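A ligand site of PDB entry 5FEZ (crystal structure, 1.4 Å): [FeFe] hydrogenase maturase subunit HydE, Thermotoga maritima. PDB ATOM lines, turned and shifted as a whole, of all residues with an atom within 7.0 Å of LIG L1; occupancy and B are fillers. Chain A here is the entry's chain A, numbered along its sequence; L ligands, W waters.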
ATOM      1  N   ILE A  66     -16.553  17.668  27.855  1.00  0.00           N
ATOM      2  CA  ILE A  66     -15.155  17.936  28.120  1.00  0.00           C
ATOM      3  C   ILE A  66     -14.733  17.359  29.470  1.00  0.00           C
ATOM      4  O   ILE A  66     -15.385  17.602  30.492  1.00  0.00           O
ATOM      5  CB  ILE A  66     -14.819  19.455  27.930  1.00  0.00           C
ATOM      6  CG1 ILE A  66     -13.314  19.646  28.090  1.00  0.00           C
ATOM      7  CG2 ILE A  66     -15.583  20.333  28.834  1.00  0.00           C
ATOM      8  CD1 ILE A  66     -12.816  21.018  27.558  1.00  0.00           C
ATOM      9  N   GLU A  68     -11.482  17.590  31.796  1.00  0.00           N
ATOM     10  CA  GLU A  68     -10.264  18.342  32.071  1.00  0.00           C
ATOM     11  C   GLU A  68      -9.459  17.474  33.038  1.00  0.00           C
ATOM     12  O   GLU A  68      -9.667  17.450  34.243  1.00  0.00           O
ATOM     13  CB  GLU A  68     -10.602  19.689  32.679  1.00  0.00           C
ATOM     14  CG  GLU A  68     -11.518  20.513  31.827  1.00  0.00           C
ATOM     15  CD  GLU A  68     -12.379  21.520  32.623  1.00  0.00           C
ATOM     16  OE1 GLU A  68     -12.814  21.162  33.723  1.00  0.00           O
ATOM     17  OE2 GLU A  68     -12.645  22.588  32.082  1.00  0.00           O
ATOM     18  N   VAL A 115     -14.155  15.399  24.563  1.00  0.00           N
ATOM     19  CA  VAL A 115     -13.014  16.284  24.503  1.00  0.00           C
ATOM     20  C   VAL A 115     -12.135  16.033  25.720  1.00  0.00           C
ATOM     21  O   VAL A 115     -12.598  16.103  26.846  1.00  0.00           O
ATOM     22  CB  VAL A 115     -13.423  17.757  24.488  1.00  0.00           C
ATOM     23  CG1 VAL A 115     -12.178  18.661  24.391  1.00  0.00           C
ATOM     24  CG2 VAL A 115     -14.409  18.070  23.380  1.00  0.00           C
ATOM     25  N   GLN A 117      -9.011  17.545  27.631  1.00  0.00           N
ATOM     26  CA  GLN A 117      -8.262  18.768  27.765  1.00  0.00           C
ATOM     27  C   GLN A 117      -7.408  18.699  28.993  1.00  0.00           C
ATOM     28  O   GLN A 117      -7.816  18.183  30.030  1.00  0.00           O
ATOM     29  CB  GLN A 117      -9.172  20.028  27.773  1.00  0.00           C
ATOM     30  CG  GLN A 117      -8.374  21.333  27.658  1.00  0.00           C
ATOM     31  CD  GLN A 117      -9.253  22.539  27.708  1.00  0.00           C
ATOM     32  OE1 GLN A 117      -9.608  22.987  28.796  1.00  0.00           O
ATOM     33  NE2 GLN A 117      -9.589  23.077  26.595  1.00  0.00           N
ATOM     34  N   SER A 146      -7.220  18.428  23.293  1.00  0.00           N
ATOM     35  CA  SER A 146      -6.853  19.852  23.546  1.00  0.00           C
ATOM     36  C   SER A 146      -5.744  19.837  24.600  1.00  0.00           C
ATOM     37  O   SER A 146      -5.965  20.110  25.748  1.00  0.00           O
ATOM     38  CB  SER A 146      -8.060  20.634  24.026  1.00  0.00           C
ATOM     39  OG  SER A 146      -7.794  22.014  24.116  1.00  0.00           O
ATOM     40  N   LEU A 167      -8.139  20.833  19.280  1.00  0.00           N
ATOM     41  CA  LEU A 167      -8.398  22.249  19.565  1.00  0.00           C
ATOM     42  C   LEU A 167      -7.133  22.894  20.014  1.00  0.00           C
ATOM     43  O   LEU A 167      -6.569  22.466  20.988  1.00  0.00           O
ATOM     44  CB  LEU A 167      -9.418  22.400  20.680  1.00  0.00           C
ATOM     45  CG  LEU A 167     -10.735  21.630  20.520  1.00  0.00           C
ATOM     46  CD1 LEU A 167     -11.649  21.837  21.724  1.00  0.00           C
ATOM     47  CD2 LEU A 167     -11.407  22.005  19.243  1.00  0.00           C
ATOM     48  N   ARG A 169      -6.362  26.853  20.306  1.00  0.00           N
ATOM     49  CA  ARG A 169      -6.663  28.233  20.018  1.00  0.00           C
ATOM     50  C   ARG A 169      -5.425  28.942  19.604  1.00  0.00           C
ATOM     51  O   ARG A 169      -4.384  28.791  20.238  1.00  0.00           O
ATOM     52  CB  ARG A 169      -7.280  28.903  21.198  1.00  0.00           C
ATOM     53  CG  ARG A 169      -8.724  28.440  21.463  1.00  0.00           C
ATOM     54  CD  ARG A 169      -9.225  29.320  22.549  1.00  0.00           C
ATOM     55  NE  ARG A 169     -10.559  28.948  22.931  1.00  0.00           N
ATOM     56  CZ  ARG A 169     -11.289  29.683  23.745  1.00  0.00           C
ATOM     57  NH1 ARG A 169     -10.820  30.824  24.302  1.00  0.00           N
ATOM     58  NH2 ARG A 169     -12.519  29.348  23.972  1.00  0.00           N
ATOM     59  N   ALA A 206      -9.200  26.489  16.026  1.00  0.00           N
ATOM     60  CA  ALA A 206      -8.404  27.649  16.466  1.00  0.00           C
ATOM     61  C   ALA A 206      -9.287  28.607  17.225  1.00  0.00           C
ATOM     62  O   ALA A 206     -10.280  28.142  17.807  1.00  0.00           O
ATOM     63  CB  ALA A 206      -7.652  28.272  15.287  1.00  0.00           C
ATOM     64  N   VAL A 235     -13.923  27.061  15.675  1.00  0.00           N
ATOM     65  CA  VAL A 235     -13.382  28.333  16.149  1.00  0.00           C
ATOM     66  C   VAL A 235     -13.928  28.605  17.529  1.00  0.00           C
ATOM     67  O   VAL A 235     -15.156  28.815  17.672  1.00  0.00           O
ATOM     68  CB  VAL A 235     -13.693  29.510  15.251  1.00  0.00           C
ATOM     69  CG1 VAL A 235     -13.063  30.766  15.808  1.00  0.00           C
ATOM     70  CG2 VAL A 235     -13.198  29.245  13.839  1.00  0.00           C
ATOM     71  N   GLY A 236     -13.076  28.602  18.558  1.00  0.00           N
ATOM     72  CA  GLY A 236     -13.450  28.896  19.924  1.00  0.00           C
ATOM     73  C   GLY A 236     -13.015  30.291  20.321  1.00  0.00           C
ATOM     74  O   GLY A 236     -11.861  30.625  20.294  1.00  0.00           O
ATOM     75  N   ILE A 237     -14.033  31.099  20.715  1.00  0.00           N
ATOM     76  CA  ILE A 237     -13.812  32.505  21.047  1.00  0.00           C
ATOM     77  C   ILE A 237     -14.453  32.796  22.385  1.00  0.00           C
ATOM     78  O   ILE A 237     -15.589  32.387  22.672  1.00  0.00           O
ATOM     79  CB  ILE A 237     -14.413  33.436  19.974  1.00  0.00           C
ATOM     80  CG1 ILE A 237     -13.573  33.326  18.699  1.00  0.00           C
ATOM     81  CG2 ILE A 237     -14.420  34.880  20.423  1.00  0.00           C
ATOM     82  CD1 ILE A 237     -14.215  33.907  17.475  1.00  0.00           C
ATOM     83  N   GLY A 238     -13.737  33.481  23.259  1.00  0.00           N
ATOM     84  CA  GLY A 238     -14.310  33.949  24.486  1.00  0.00           C
ATOM     85  C   GLY A 238     -13.606  35.230  24.944  1.00  0.00           C
ATOM     86  O   GLY A 238     -12.530  35.576  24.438  1.00  0.00           O
ATOM     87  N   PRO A 239     -14.193  35.849  25.952  1.00  0.00           N
ATOM     88  CA  PRO A 239     -13.563  37.032  26.544  1.00  0.00           C
ATOM     89  C   PRO A 239     -12.443  36.652  27.445  1.00  0.00           C
ATOM     90  O   PRO A 239     -12.463  35.616  28.099  1.00  0.00           O
ATOM     91  CB  PRO A 239     -14.686  37.649  27.383  1.00  0.00           C
ATOM     92  CG  PRO A 239     -15.456  36.433  27.840  1.00  0.00           C
ATOM     93  CD  PRO A 239     -15.438  35.542  26.647  1.00  0.00           C
ATOM     94  N   PRO A 276     -18.362  26.980  19.082  1.00  0.00           N
ATOM     95  CA  PRO A 276     -19.007  26.847  20.387  1.00  0.00           C
ATOM     96  C   PRO A 276     -19.478  28.111  21.024  1.00  0.00           C
ATOM     97  O   PRO A 276     -18.951  29.224  20.758  1.00  0.00           O
ATOM     98  CB  PRO A 276     -17.920  26.196  21.273  1.00  0.00           C
ATOM     99  CG  PRO A 276     -16.693  26.756  20.745  1.00  0.00           C
ATOM    100  CD  PRO A 276     -16.874  26.650  19.261  1.00  0.00           C
ATOM    101  N   ALA A 277     -20.483  28.031  21.842  1.00  0.00           N
ATOM    102  CA  ALA A 277     -20.908  29.026  22.808  1.00  0.00           C
ATOM    103  C   ALA A 277     -20.151  28.727  24.087  1.00  0.00           C
ATOM    104  O   ALA A 277     -20.469  27.779  24.768  1.00  0.00           O
ATOM    105  CB  ALA A 277     -22.425  28.977  23.042  1.00  0.00           C
ATOM    106  N   THR A 278     -19.043  29.421  24.326  1.00  0.00           N
ATOM    107  CA  THR A 278     -18.085  29.003  25.311  1.00  0.00           C
ATOM    108  C   THR A 278     -18.514  29.274  26.734  1.00  0.00           C
ATOM    109  O   THR A 278     -19.249  30.131  26.985  1.00  0.00           O
ATOM    110  CB  THR A 278     -16.716  29.637  25.040  1.00  0.00           C
ATOM    111  OG1 THR A 278     -16.829  31.053  25.133  1.00  0.00           O
ATOM    112  CG2 THR A 278     -16.184  29.262  23.649  1.00  0.00           C
ATOM    113  N   THR A 279     -17.995  28.466  27.646  1.00  0.00           N
ATOM    114  CA  THR A 279     -18.273  28.641  29.070  1.00  0.00           C
ATOM    115  C   THR A 279     -17.838  30.030  29.534  1.00  0.00           C
ATOM    116  O   THR A 279     -18.475  30.604  30.345  1.00  0.00           O
ATOM    117  CB  THR A 279     -17.599  27.517  29.887  1.00  0.00           C
ATOM    118  OG1 THR A 279     -18.285  26.276  29.586  1.00  0.00           O
ATOM    119  CG2 THR A 279     -17.798  27.775  31.370  1.00  0.00           C
ATOM    120  N   ALA A 280     -16.763  30.580  28.958  1.00  0.00           N
ATOM    121  CA  ALA A 280     -16.345  31.936  29.329  1.00  0.00           C
ATOM    122  C   ALA A 280     -17.420  32.975  29.029  1.00  0.00           C
ATOM    123  O   ALA A 280     -17.638  33.852  29.807  1.00  0.00           O
ATOM    124  CB  ALA A 280     -15.023  32.289  28.696  1.00  0.00           C
ATOM    125  N   MET A 281     -18.128  32.827  27.913  1.00  0.00           N
ATOM    126  CA  MET A 281     -19.271  33.670  27.609  1.00  0.00           C
ATOM    127  C   MET A 281     -20.393  33.549  28.684  1.00  0.00           C
ATOM    128  O   MET A 281     -20.978  34.504  29.017  1.00  0.00           O
ATOM    129  CB  MET A 281     -19.841  33.373  26.216  1.00  0.00           C
ATOM    130  CG  MET A 281     -18.913  33.823  25.074  1.00  0.00           C
ATOM    131  SD  MET A 281     -18.699  35.582  25.022  1.00  0.00           S
ATOM    132  CE  MET A 281     -19.811  36.026  23.727  1.00  0.00           C
ATOM    133  N   THR A 283     -19.866  32.770  31.759  1.00  0.00           N
ATOM    134  CA  THR A 283     -19.273  33.235  33.001  1.00  0.00           C
ATOM    135  C   THR A 283     -19.322  34.765  33.122  1.00  0.00           C
ATOM    136  O   THR A 283     -19.677  35.213  34.209  1.00  0.00           O
ATOM    137  CB  THR A 283     -17.808  32.682  33.119  1.00  0.00           C
ATOM    138  OG1 THR A 283     -17.857  31.269  33.124  1.00  0.00           O
ATOM    139  CG2 THR A 283     -17.145  33.194  34.417  1.00  0.00           C
ATOM    140  N   MET A 301     -20.268  22.852  25.025  1.00  0.00           N
ATOM    141  CA  MET A 301     -19.300  21.990  25.643  1.00  0.00           C
ATOM    142  C   MET A 301     -19.554  21.832  27.163  1.00  0.00           C
ATOM    143  O   MET A 301     -18.827  22.409  27.925  1.00  0.00           O
ATOM    144  CB  MET A 301     -17.887  22.491  25.268  1.00  0.00           C
ATOM    145  CG  MET A 301     -17.761  22.698  23.718  1.00  0.00           C
ATOM    146  SD  MET A 301     -16.241  23.463  23.094  1.00  0.00           S
ATOM    147  CE  MET A 301     -15.325  22.039  23.432  1.00  0.00           C
ATOM    148  N   LEU A 315      -9.133  28.173  34.755  1.00  0.00           N
ATOM    149  CA  LEU A 315      -8.298  28.976  33.909  1.00  0.00           C
ATOM    150  C   LEU A 315      -8.557  30.440  34.243  1.00  0.00           C
ATOM    151  O   LEU A 315      -7.682  31.253  34.207  1.00  0.00           O
ATOM    152  CB  LEU A 315      -8.659  28.731  32.437  1.00  0.00           C
ATOM    153  CG  LEU A 315      -8.673  27.267  32.015  1.00  0.00           C
ATOM    154  CD1 LEU A 315      -8.989  27.141  30.546  1.00  0.00           C
ATOM    155  CD2 LEU A 315      -7.457  26.618  32.382  1.00  0.00           C
ATOM    156  N   TYR A 316      -9.808  30.719  34.548  1.00  0.00           N
ATOM    157  CA  TYR A 316     -10.306  32.026  34.937  1.00  0.00           C
ATOM    158  C   TYR A 316     -11.281  31.775  36.086  1.00  0.00           C
ATOM    159  O   TYR A 316     -11.802  30.716  36.208  1.00  0.00           O
ATOM    160  CB  TYR A 316     -10.986  32.773  33.775  1.00  0.00           C
ATOM    161  CG  TYR A 316     -12.023  31.938  33.031  1.00  0.00           C
ATOM    162  CD1 TYR A 316     -13.315  31.811  33.517  1.00  0.00           C
ATOM    163  CD2 TYR A 316     -11.696  31.240  31.888  1.00  0.00           C
ATOM    164  CE1 TYR A 316     -14.243  31.050  32.876  1.00  0.00           C
ATOM    165  CE2 TYR A 316     -12.628  30.452  31.253  1.00  0.00           C
ATOM    166  CZ  TYR A 316     -13.872  30.376  31.741  1.00  0.00           C
ATOM    167  OH  TYR A 316     -14.784  29.601  31.145  1.00  0.00           O
ATOM    168  N   LYS A 319     -15.882  30.256  37.060  1.00  0.00           N
ATOM    169  CA  LYS A 319     -16.385  29.305  36.127  1.00  0.00           C
ATOM    170  C   LYS A 319     -17.722  28.714  36.636  1.00  0.00           C
ATOM    171  O   LYS A 319     -17.894  28.283  37.722  1.00  0.00           O
ATOM    172  CB  LYS A 319     -15.344  28.263  35.941  1.00  0.00           C
ATOM    173  CG  LYS A 319     -15.414  27.553  34.610  1.00  0.00           C
ATOM    174  CD  LYS A 319     -14.447  26.425  34.739  1.00  0.00           C
HETATM  175  C1  LIG L   1     -13.317  25.785  25.147  1.00  0.00           C
HETATM  176  C2  LIG L   1     -12.030  27.228  27.053  1.00  0.00           C
HETATM  177  O1  LIG L   1     -13.872  27.036  23.290  1.00  0.00           O
HETATM  178  C3  LIG L   1     -13.532  25.964  23.667  1.00  0.00           C
HETATM  179  O2  LIG L   1     -13.238  25.061  22.856  1.00  0.00           O
HETATM  180  N1  LIG L   1     -14.130  26.691  25.949  1.00  0.00           N
HETATM  181  C4  LIG L   1     -13.595  24.319  25.574  1.00  0.00           C
HETATM  182 SE1  LIG L   1     -11.454  26.115  25.542  1.00  0.00          SE
HETATM  183  C5  LIG L   1     -13.455  26.942  27.271  1.00  0.00           C
HETATM  184  C6  LIG L   1     -14.139  28.043  28.078  1.00  0.00           C
HETATM  185  O3  LIG L   1     -14.023  27.862  29.325  1.00  0.00           O
HETATM  186  O4  LIG L   1     -14.682  28.960  27.626  1.00  0.00           O
HETATM  187  N1  LG2 L   2      -9.697  34.110  30.521  1.00  0.00           N
HETATM  188  C1  LG2 L   2     -10.398  33.574  29.506  1.00  0.00           C
HETATM  189  N2  LG2 L   2      -9.991  32.530  28.764  1.00  0.00           N
HETATM  190  C2  LG2 L   2      -8.866  31.953  29.101  1.00  0.00           C
HETATM  191  N3  LG2 L   2      -8.241  30.907  28.618  1.00  0.00           N
HETATM  192  C3  LG2 L   2      -7.144  30.731  29.377  1.00  0.00           C
HETATM  193  N4  LG2 L   2      -7.068  31.611  30.331  1.00  0.00           N
HETATM  194  C4  LG2 L   2      -8.152  32.415  30.216  1.00  0.00           C
HETATM  195  C5  LG2 L   2      -8.611  33.547  30.925  1.00  0.00           C
HETATM  196  N5  LG2 L   2      -7.953  34.066  31.996  1.00  0.00           N
HETATM  197  C6  LG2 L   2      -8.595  30.256  27.364  1.00  0.00           C
HETATM  198  C7  LG2 L   2      -7.453  30.242  26.350  1.00  0.00           C
HETATM  199  C8  LG2 L   2      -7.227  28.768  26.143  1.00  0.00           C
HETATM  200  C9  LG2 L   2      -8.593  28.183  26.407  1.00  0.00           C
HETATM  201  C10 LG2 L   2      -8.525  26.780  26.921  1.00  0.00           C
HETATM  202  O1  LG2 L   2      -8.970  28.918  27.582  1.00  0.00           O
HETATM  203  O2  LG2 L   2      -7.926  30.901  25.165  1.00  0.00           O
HETATM  204  O3  LG2 L   2      -6.826  28.389  24.809  1.00  0.00           O
HETATM  205  N1  LG3 L   3      -2.982  23.897  27.482  1.00  0.00           N
HETATM  206  C1  LG3 L   3      -3.749  23.720  26.229  1.00  0.00           C
HETATM  207  C2  LG3 L   3      -3.651  24.985  25.383  1.00  0.00           C
HETATM  208  O1  LG3 L   3      -3.940  24.981  24.205  1.00  0.00           O
HETATM  209  C3  LG3 L   3      -5.184  23.389  26.595  1.00  0.00           C
HETATM  210  C4  LG3 L   3      -6.049  24.620  26.859  1.00  0.00           C
HETATM  211  S1  LG3 L   3      -5.482  25.625  28.237  1.00  0.00           S
HETATM  212  C5  LG3 L   3      -5.965  24.390  29.509  1.00  0.00           C
HETATM  213  O2  LG3 L   3      -3.196  25.974  26.063  1.00  0.00           O
HETATM  214  O   HOH W   1     -13.737  30.895  25.905  1.00  0.00           O
HETATM  215  O   HOH W   2     -10.766  25.882  21.916  1.00  0.00           O
HETATM  216  O   HOH W   3     -16.781  26.015  26.573  1.00  0.00           O
HETATM  217  O   HOH W   4     -13.602  25.205  19.966  1.00  0.00           O
HETATM  218  O   HOH W   5     -12.314  26.588  30.715  1.00  0.00           O
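OH of Tyr 316 lies within hydrogen-bond range of N of Ala 280 (3.1 Å). The guanidinium group (NE) of Arg 169 sits at hydrogen-bond distance from the backbone carbonyl oxygen (O) of Gly 236, at 3.4 Å. OG1 of Thr 278 lies within hydrogen-bond range of O of Ile 237, 3.1 Å away. The side-chain hydroxyl (OG1) of Thr 283 sits at hydrogen-bond distance from the backbone carbonyl oxygen (O) of Thr 279 (2.9 Å). OG of Ser 146 lies within hydrogen-bond range of NE2 of Gln 117, at 3.2 Å. The backbone carbonyl oxygen (O) of Leu 167 sits at hydrogen-bond distance from the side-chain hydroxyl (OG) of Ser 146. The backbone carbonyl oxygen (O) of Ala 206 is in hydrogen-bond range of the backbone NH (N) of Gly 236 (2.9 Å).
Water W1 lies within hydrogen-bond range of an oxygen (O4) of LIG L1, the guanidinium group (NH2) of Arg 169 and the side-chain hydroxyl (OG1) of Thr 278. Water W2 bridges an oxygen (O2) of LIG L1 (2.8 Å) and the guanidinium group of Arg 169 (3.2 Å). Water W3 bridges a nitrogen (N1) of LIG L1 (2.8 Å) and the backbone NH of Thr 279 (2.9 Å).
SD of Met 301 lies close to O2 of LIG L1 (3.4 Å). Residues that only touch LIG L1: Thr 278, Gln 117, Leu 167, Pro 276, Gly 236 and Ile 66. Hydrophobic or aromatic side chains within 4 Å of LIG L1: Ile 66, Leu 167, Pro 276, Ala 280, Met 301 and Tyr 316. Within 4 Å of LIG L1: Ile 66, Gln 117, Leu 167, Arg 169, Gly 236, Pro 276, Thr 278, Thr 279, Ala 280, Met 301 and Tyr 316.
The side-chain hydroxyl (OH) of Tyr 316 lies within hydrogen-bond range of an oxygen (O3) of LIG L1 (2.6 Å). The guanidinium group (NH2) of Arg 169 is in salt-bridge range of an oxygen (O1) of LIG L1, at 2.8 Å. N of Ala 280 is in hydrogen-bond range of O4 of LIG L1 (3.0 Å). An oxygen (O4) of LIG L1 is in hydrogen-bond range of the backbone NH (N) of Thr 279 (3.3 Å). An oxygen (O2) of LG2 L2 is in hydrogen-bond range of the guanidinium group (NH1) of Arg 169 (3.0 Å).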
